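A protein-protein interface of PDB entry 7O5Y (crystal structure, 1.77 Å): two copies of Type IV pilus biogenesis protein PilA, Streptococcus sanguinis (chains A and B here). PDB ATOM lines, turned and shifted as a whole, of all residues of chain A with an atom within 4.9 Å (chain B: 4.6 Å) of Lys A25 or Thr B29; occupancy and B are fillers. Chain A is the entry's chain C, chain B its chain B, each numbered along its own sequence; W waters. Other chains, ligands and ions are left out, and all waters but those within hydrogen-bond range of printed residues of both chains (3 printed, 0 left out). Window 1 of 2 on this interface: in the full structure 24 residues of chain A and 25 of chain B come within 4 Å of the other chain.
Water W1 lies within hydrogen-bond range of the backbone carbonyl oxygen of Gly B133 (2.7 Å), the side-chain hydroxyl of Tyr A115 (3.2 Å) and the side-chain hydroxyl of Tyr B115 (3.3 Å).
Water W3 bridges the side-chain hydroxyl of Ser B30 and the side-chain hydroxyl of Tyr A26.
Water W2 lies within hydrogen-bond range of the side-chain hydroxyl of Tyr A115 (3.0 Å), the side-chain amino group of Lys A25 (3.3 Å) and the backbone NH of Gly B133 (3.3 Å).
Of the 12 printed residues of chain B, 8 touch a printed residue of chain A.
Hydrophobic or aromatic side chains of chain A that line the printed part of chain B: Tyr A21, Leu A22, Tyr A26 and Tyr A115.
Along chain A the printed residues that touch a printed residue of chain B span positions 21 to 115.
Lys A25 touches Thr B29, and with the chains exchanged Thr A29 touches Lys B25.
Lys A25 touches Tyr B115, and with the chains exchanged Tyr A115 touches Lys B25.
Tyr A26 touches its own counterpart, Tyr B26.
Tyr A26 touches Thr B29, but with the chains exchanged Thr A29 does not touch Tyr B26 (4.3 Å).
Positions printed for both chains: 25, 26, 27, 28, 29 and 115.
Of the 15 pairs that touch across the chains among the printed residues, 6 have their exchanged pair printed and touching as well.
Among the printed residues, merely in contact across the chains: Leu A22 with Thr B29, Leu A22 with Thr B32, Leu A22 with Gln B33, Leu A22 with His B117, Lys A25 with Lys B25, Lys A25 with Thr B29, Tyr A26 with Tyr B26, Tyr A26 with Thr B29, Tyr A26 with Ser B30 and Thr A29 with Lys B25.
Lys A25 touches just these residues of chain B: Lys B25 (3.7 Å), Thr B29 (3.1 Å), Tyr B115 (2.7 Å) and His B117 (3.0 Å).
Of chain A, only Leu A22 (3.98 Å), Lys A25 (3.1 Å) and Tyr A26 (3.4 Å) come within 4 Å of Thr B29.
Of the printed residues of chain A, Gln B33 touches Leu A22 and Tyr A26.
Of the printed residues of chain A, His B117 touches Tyr A21, Leu A22 and Lys A25.
Printed residues of chain A within 4 Å of Lys B25: Lys A25, Thr A29 and Tyr A115.
Thr B27 touches none of the printed residues of chain A.
The nearest residue of chain B that does not touch Lys A25 is Gly B133 (4.3 Å).
The nearest printed residue of chain A that does not touch Thr B29 is Thr A29 (5.5 Å).
The nearest printed residue of chain A that does not touch Thr B32 is Tyr A21 (6.0 Å).
NE2 of His B117 sits at hydrogen-bond distance from OH of Tyr A21, at 2.8 Å.
The side-chain hydroxyl of Tyr A26 is in hydrogen-bond range of the side-chain amide oxygen of Gln B33, at 2.6 Å.
NE2 of His B117 lies close to NZ of Lys A25, 3.3 Å away.
The side-chain amino group of Lys B25 is in hydrogen-bond range of the side-chain hydroxyl of Tyr A115 (2.8 Å).
The side-chain hydroxyl (OH) of Tyr B115 sits at hydrogen-bond distance from the side-chain amino group (NZ) of Lys A25, 2.7 Å away.
The side-chain hydroxyl (OG1) of Thr B32 is in hydrogen-bond range of the backbone carbonyl oxygen (O) of Ala B28 (3.3 Å).
The side-chain hydroxyl (OG1) of Thr B32 lies within hydrogen-bond range of a ring nitrogen (ND1) of His B117 (2.8 Å).
The side-chain hydroxyl (OG1) of Thr A29 sits at hydrogen-bond distance from the backbone carbonyl oxygen (O) of Lys A25, 2.8 Å away.
OH of Tyr B115 lies within hydrogen-bond range of NZ of Lys B25, 2.9 Å away.
The backbone carbonyl oxygen (O) of Tyr B26 lies within hydrogen-bond range of the side-chain hydroxyl (OG) of Ser B30 (3.0 Å).
OG1 of Thr B29 is in hydrogen-bond range of O of Lys B25, at 2.8 Å.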
ATOM      1  N   TYR A  21     -19.299   0.780  24.157  1.00  0.00           N
ATOM      2  CA  TYR A  21     -19.532  -0.359  23.277  1.00  0.00           C
ATOM      3  C   TYR A  21     -18.964  -0.093  21.890  1.00  0.00           C
ATOM      4  O   TYR A  21     -18.275  -0.941  21.309  1.00  0.00           O
ATOM      5  CB  TYR A  21     -21.037  -0.663  23.207  1.00  0.00           C
ATOM      6  CG  TYR A  21     -21.479  -1.375  21.942  1.00  0.00           C
ATOM      7  CD1 TYR A  21     -21.194  -2.722  21.746  1.00  0.00           C
ATOM      8  CD2 TYR A  21     -22.206  -0.712  20.951  1.00  0.00           C
ATOM      9  CE1 TYR A  21     -21.590  -3.383  20.592  1.00  0.00           C
ATOM     10  CE2 TYR A  21     -22.617  -1.372  19.791  1.00  0.00           C
ATOM     11  CZ  TYR A  21     -22.313  -2.703  19.622  1.00  0.00           C
ATOM     12  OH  TYR A  21     -22.694  -3.368  18.478  1.00  0.00           O
ATOM     13  N   LEU A  22     -19.230   1.099  21.350  1.00  0.00           N
ATOM     14  CA  LEU A  22     -18.711   1.437  20.031  1.00  0.00           C
ATOM     15  C   LEU A  22     -17.190   1.455  20.035  1.00  0.00           C
ATOM     16  O   LEU A  22     -16.557   0.981  19.089  1.00  0.00           O
ATOM     17  CB  LEU A  22     -19.275   2.787  19.577  1.00  0.00           C
ATOM     18  CG  LEU A  22     -20.803   2.821  19.453  1.00  0.00           C
ATOM     19  CD1 LEU A  22     -21.282   4.253  19.213  1.00  0.00           C
ATOM     20  CD2 LEU A  22     -21.304   1.899  18.344  1.00  0.00           C
ATOM     21  N   LYS A  23     -16.584   1.988  21.098  1.00  0.00           N
ATOM     22  CA  LYS A  23     -15.126   2.041  21.156  1.00  0.00           C
ATOM     23  C   LYS A  23     -14.520   0.646  21.246  1.00  0.00           C
ATOM     24  O   LYS A  23     -13.482   0.371  20.626  1.00  0.00           O
ATOM     25  CB  LYS A  23     -14.677   2.900  22.338  1.00  0.00           C
ATOM     26  CG  LYS A  23     -14.905   4.382  22.114  1.00  0.00           C
ATOM     27  CD  LYS A  23     -14.117   5.244  23.086  1.00  0.00           C
ATOM     28  CE  LYS A  23     -14.644   5.125  24.504  1.00  0.00           C
ATOM     29  NZ  LYS A  23     -13.838   5.958  25.440  1.00  0.00           N
ATOM     30  N   ALA A  24     -15.143  -0.241  22.025  1.00  0.00           N
ATOM     31  CA  ALA A  24     -14.656  -1.615  22.092  1.00  0.00           C
ATOM     32  C   ALA A  24     -14.822  -2.326  20.757  1.00  0.00           C
ATOM     33  O   ALA A  24     -13.981  -3.148  20.383  1.00  0.00           O
ATOM     34  CB  ALA A  24     -15.380  -2.378  23.200  1.00  0.00           C
ATOM     35  N   LYS A  25     -15.892  -2.018  20.021  1.00  0.00           N
ATOM     36  CA  LYS A  25     -16.038  -2.575  18.684  1.00  0.00           C
ATOM     37  C   LYS A  25     -14.951  -2.053  17.749  1.00  0.00           C
ATOM     38  O   LYS A  25     -14.393  -2.823  16.963  1.00  0.00           O
ATOM     39  CB  LYS A  25     -17.430  -2.267  18.122  1.00  0.00           C
ATOM     40  CG  LYS A  25     -17.659  -2.851  16.735  1.00  0.00           C
ATOM     41  CD  LYS A  25     -19.109  -2.740  16.269  1.00  0.00           C
ATOM     42  CE  LYS A  25     -19.238  -3.422  14.898  1.00  0.00           C
ATOM     43  NZ  LYS A  25     -20.621  -3.696  14.495  1.00  0.00           N
ATOM     44  N   TYR A  26     -14.636  -0.753  17.821  1.00  0.00           N
ATOM     45  CA  TYR A  26     -13.523  -0.216  17.033  1.00  0.00           C
ATOM     46  C   TYR A  26     -12.233  -0.954  17.348  1.00  0.00           C
ATOM     47  O   TYR A  26     -11.485  -1.342  16.446  1.00  0.00           O
ATOM     48  CB  TYR A  26     -13.283   1.267  17.327  1.00  0.00           C
ATOM     49  CG  TYR A  26     -14.333   2.262  16.932  1.00  0.00           C
ATOM     50  CD1 TYR A  26     -14.979   2.200  15.700  1.00  0.00           C
ATOM     51  CD2 TYR A  26     -14.643   3.308  17.788  1.00  0.00           C
ATOM     52  CE1 TYR A  26     -15.938   3.153  15.356  1.00  0.00           C
ATOM     53  CE2 TYR A  26     -15.596   4.245  17.465  1.00  0.00           C
ATOM     54  CZ  TYR A  26     -16.242   4.167  16.254  1.00  0.00           C
ATOM     55  OH  TYR A  26     -17.186   5.122  15.959  1.00  0.00           O
ATOM     56  N   THR A  27     -11.927  -1.089  18.641  1.00  0.00           N
ATOM     57  CA  THR A  27     -10.640  -1.653  19.035  1.00  0.00           C
ATOM     58  C   THR A  27     -10.545  -3.114  18.628  1.00  0.00           C
ATOM     59  O   THR A  27      -9.517  -3.551  18.106  1.00  0.00           O
ATOM     60  CB  THR A  27     -10.423  -1.489  20.543  1.00  0.00           C
ATOM     61  OG1 THR A  27     -10.328  -0.095  20.868  1.00  0.00           O
ATOM     62  CG2 THR A  27      -9.120  -2.182  20.979  1.00  0.00           C
ATOM     63  N   ALA A  28     -11.622  -3.876  18.823  1.00  0.00           N
ATOM     64  CA  ALA A  28     -11.618  -5.269  18.392  1.00  0.00           C
ATOM     65  C   ALA A  28     -11.398  -5.382  16.889  1.00  0.00           C
ATOM     66  O   ALA A  28     -10.621  -6.229  16.431  1.00  0.00           O
ATOM     67  CB  ALA A  28     -12.927  -5.947  18.800  1.00  0.00           C
ATOM     68  N   THR A  29     -12.071  -4.533  16.104  1.00  0.00           N
ATOM     69  CA  THR A  29     -11.904  -4.556  14.655  1.00  0.00           C
ATOM     70  C   THR A  29     -10.474  -4.216  14.259  1.00  0.00           C
ATOM     71  O   THR A  29      -9.893  -4.865  13.382  1.00  0.00           O
ATOM     72  CB  THR A  29     -12.891  -3.577  14.009  1.00  0.00           C
ATOM     73  OG1 THR A  29     -14.223  -3.939  14.399  1.00  0.00           O
ATOM     74  CG2 THR A  29     -12.777  -3.605  12.480  1.00  0.00           C
ATOM     75  N   TYR A 115     -16.332  -6.686  23.526  1.00  0.00           N
ATOM     76  CA  TYR A 115     -16.720  -6.964  22.151  1.00  0.00           C
ATOM     77  C   TYR A 115     -15.765  -7.998  21.574  1.00  0.00           C
ATOM     78  O   TYR A 115     -14.543  -7.857  21.700  1.00  0.00           O
ATOM     79  CB  TYR A 115     -16.717  -5.701  21.288  1.00  0.00           C
ATOM     80  CG  TYR A 115     -17.320  -5.950  19.925  1.00  0.00           C
ATOM     81  CD1 TYR A 115     -16.552  -6.456  18.890  1.00  0.00           C
ATOM     82  CD2 TYR A 115     -18.666  -5.709  19.689  1.00  0.00           C
ATOM     83  CE1 TYR A 115     -17.098  -6.703  17.655  1.00  0.00           C
ATOM     84  CE2 TYR A 115     -19.219  -5.958  18.465  1.00  0.00           C
ATOM     85  CZ  TYR A 115     -18.437  -6.447  17.449  1.00  0.00           C
ATOM     86  OH  TYR A 115     -18.988  -6.693  16.216  1.00  0.00           O
ATOM     87  N   LYS B  25     -16.552  -2.384   8.169  1.00  0.00           N
ATOM     88  CA  LYS B  25     -17.037  -2.579   9.532  1.00  0.00           C
ATOM     89  C   LYS B  25     -16.711  -1.370  10.395  1.00  0.00           C
ATOM     90  O   LYS B  25     -17.542  -0.915  11.188  1.00  0.00           O
ATOM     91  CB  LYS B  25     -16.424  -3.852  10.134  1.00  0.00           C
ATOM     92  CG  LYS B  25     -16.858  -4.167  11.571  1.00  0.00           C
ATOM     93  CD  LYS B  25     -16.234  -5.497  12.053  1.00  0.00           C
ATOM     94  CE  LYS B  25     -16.604  -5.825  13.504  1.00  0.00           C
ATOM     95  NZ  LYS B  25     -17.875  -6.588  13.603  1.00  0.00           N
ATOM     96  N   TYR B  26     -15.510  -0.822  10.231  1.00  0.00           N
ATOM     97  CA  TYR B  26     -15.117   0.347  11.002  1.00  0.00           C
ATOM     98  C   TYR B  26     -15.957   1.563  10.629  1.00  0.00           C
ATOM     99  O   TYR B  26     -16.393   2.316  11.505  1.00  0.00           O
ATOM    100  CB  TYR B  26     -13.637   0.632  10.778  1.00  0.00           C
ATOM    101  CG  TYR B  26     -12.992   1.368  11.917  1.00  0.00           C
ATOM    102  CD1 TYR B  26     -13.136   2.743  12.048  1.00  0.00           C
ATOM    103  CD2 TYR B  26     -12.233   0.693  12.862  1.00  0.00           C
ATOM    104  CE1 TYR B  26     -12.540   3.428  13.088  1.00  0.00           C
ATOM    105  CE2 TYR B  26     -11.632   1.371  13.910  1.00  0.00           C
ATOM    106  CZ  TYR B  26     -11.787   2.738  14.012  1.00  0.00           C
ATOM    107  OH  TYR B  26     -11.203   3.421  15.048  1.00  0.00           O
ATOM    108  N   THR B  27     -16.193   1.766   9.337  1.00  0.00           N
ATOM    109  CA  THR B  27     -16.952   2.936   8.906  1.00  0.00           C
ATOM    110  C   THR B  27     -18.408   2.829   9.329  1.00  0.00           C
ATOM    111  O   THR B  27     -18.998   3.807   9.800  1.00  0.00           O
ATOM    112  CB  THR B  27     -16.832   3.101   7.393  1.00  0.00           C
ATOM    113  OG1 THR B  27     -15.454   3.310   7.059  1.00  0.00           O
ATOM    114  CG2 THR B  27     -17.681   4.293   6.896  1.00  0.00           C
ATOM    115  N   ALA B  28     -18.998   1.643   9.178  1.00  0.00           N
ATOM    116  CA  ALA B  28     -20.361   1.438   9.646  1.00  0.00           C
ATOM    117  C   ALA B  28     -20.476   1.766  11.128  1.00  0.00           C
ATOM    118  O   ALA B  28     -21.407   2.460  11.550  1.00  0.00           O
ATOM    119  CB  ALA B  28     -20.802   0.000   9.366  1.00  0.00           C
ATOM    120  N   THR B  29     -19.516   1.294  11.934  1.00  0.00           N
ATOM    121  CA  THR B  29     -19.548   1.592  13.362  1.00  0.00           C
ATOM    122  C   THR B  29     -19.410   3.087  13.613  1.00  0.00           C
ATOM    123  O   THR B  29     -20.079   3.640  14.497  1.00  0.00           O
ATOM    124  CB  THR B  29     -18.442   0.819  14.088  1.00  0.00           C
ATOM    125  OG1 THR B  29     -18.546  -0.574  13.758  1.00  0.00           O
ATOM    126  CG2 THR B  29     -18.578   0.989  15.595  1.00  0.00           C
ATOM    127  N   SER B  30     -18.540   3.756  12.848  1.00  0.00           N
ATOM    128  CA  SER B  30     -18.404   5.203  12.962  1.00  0.00           C
ATOM    129  C   SER B  30     -19.711   5.908  12.639  1.00  0.00           C
ATOM    130  O   SER B  30     -20.028   6.937  13.245  1.00  0.00           O
ATOM    131  CB  SER B  30     -17.295   5.695  12.031  1.00  0.00           C
ATOM    132  OG  SER B  30     -16.040   5.138  12.395  1.00  0.00           O
ATOM    133  N   GLY B  31     -20.474   5.371  11.684  1.00  0.00           N
ATOM    134  CA  GLY B  31     -21.787   5.929  11.402  1.00  0.00           C
ATOM    135  C   GLY B  31     -22.727   5.814  12.580  1.00  0.00           C
ATOM    136  O   GLY B  31     -23.489   6.739  12.883  1.00  0.00           O
ATOM    137  N   THR B  32     -22.692   4.680  13.274  1.00  0.00           N
ATOM    138  CA  THR B  32     -23.539   4.544  14.446  1.00  0.00           C
ATOM    139  C   THR B  32     -23.166   5.564  15.508  1.00  0.00           C
ATOM    140  O   THR B  32     -24.043   6.155  16.145  1.00  0.00           O
ATOM    141  CB  THR B  32     -23.443   3.129  15.000  1.00  0.00           C
ATOM    142  OG1 THR B  32     -23.726   2.207  13.941  1.00  0.00           O
ATOM    143  CG2 THR B  32     -24.455   2.951  16.117  1.00  0.00           C
ATOM    144  N   GLN B  33     -21.867   5.794  15.702  1.00  0.00           N
ATOM    145  CA  GLN B  33     -21.454   6.797  16.677  1.00  0.00           C
ATOM    146  C   GLN B  33     -21.930   8.181  16.268  1.00  0.00           C
ATOM    147  O   GLN B  33     -22.399   8.959  17.105  1.00  0.00           O
ATOM    148  CB  GLN B  33     -19.938   6.802  16.834  1.00  0.00           C
ATOM    149  CG  GLN B  33     -19.476   7.875  17.803  1.00  0.00           C
ATOM    150  CD  GLN B  33     -17.979   7.900  17.960  1.00  0.00           C
ATOM    151  OE1 GLN B  33     -17.329   6.862  17.907  1.00  0.00           O
ATOM    152  NE2 GLN B  33     -17.420   9.091  18.152  1.00  0.00           N
ATOM    153  N   TYR B 115     -21.197  -3.767   4.891  1.00  0.00           N
ATOM    154  CA  TYR B 115     -21.332  -4.107   6.298  1.00  0.00           C
ATOM    155  C   TYR B 115     -22.461  -3.280   6.890  1.00  0.00           C
ATOM    156  O   TYR B 115     -22.530  -2.066   6.665  1.00  0.00           O
ATOM    157  CB  TYR B 115     -20.037  -3.846   7.063  1.00  0.00           C
ATOM    158  CG  TYR B 115     -20.110  -4.297   8.508  1.00  0.00           C
ATOM    159  CD1 TYR B 115     -20.611  -3.459   9.490  1.00  0.00           C
ATOM    160  CD2 TYR B 115     -19.688  -5.568   8.881  1.00  0.00           C
ATOM    161  CE1 TYR B 115     -20.686  -3.861  10.809  1.00  0.00           C
ATOM    162  CE2 TYR B 115     -19.760  -5.981  10.198  1.00  0.00           C
ATOM    163  CZ  TYR B 115     -20.256  -5.123  11.156  1.00  0.00           C
ATOM    164  OH  TYR B 115     -20.325  -5.510  12.471  1.00  0.00           O
ATOM    165  N   HIS B 117     -24.444  -2.337  10.478  1.00  0.00           N
ATOM    166  CA  HIS B 117     -24.470  -2.316  11.934  1.00  0.00           C
ATOM    167  C   HIS B 117     -25.866  -1.897  12.374  1.00  0.00           C
ATOM    168  O   HIS B 117     -26.391  -0.892  11.889  1.00  0.00           O
ATOM    169  CB  HIS B 117     -23.411  -1.337  12.450  1.00  0.00           C
ATOM    170  CG  HIS B 117     -23.172  -1.395  13.924  1.00  0.00           C
ATOM    171  ND1 HIS B 117     -22.709  -0.307  14.636  1.00  0.00           N
ATOM    172  CD2 HIS B 117     -23.314  -2.398  14.822  1.00  0.00           C
ATOM    173  CE1 HIS B 117     -22.579  -0.639  15.908  1.00  0.00           C
ATOM    174  NE2 HIS B 117     -22.938  -1.905  16.048  1.00  0.00           N
ATOM    175  N   GLY B 133     -24.145  -6.956  13.761  1.00  0.00           N
ATOM    176  CA  GLY B 133     -23.409  -6.437  12.633  1.00  0.00           C
ATOM    177  C   GLY B 133     -23.064  -7.559  11.684  1.00  0.00           C
ATOM    178  O   GLY B 133     -22.649  -8.633  12.126  1.00  0.00           O
HETATM  179  O   HOH W   1     -21.127  -8.149  14.290  1.00  0.00           O
HETATM  180  O   HOH W   2     -21.976  -6.146  16.156  1.00  0.00           O
HETATM  181  O   HOH W   3     -14.597   6.507  14.385  1.00  0.00           O
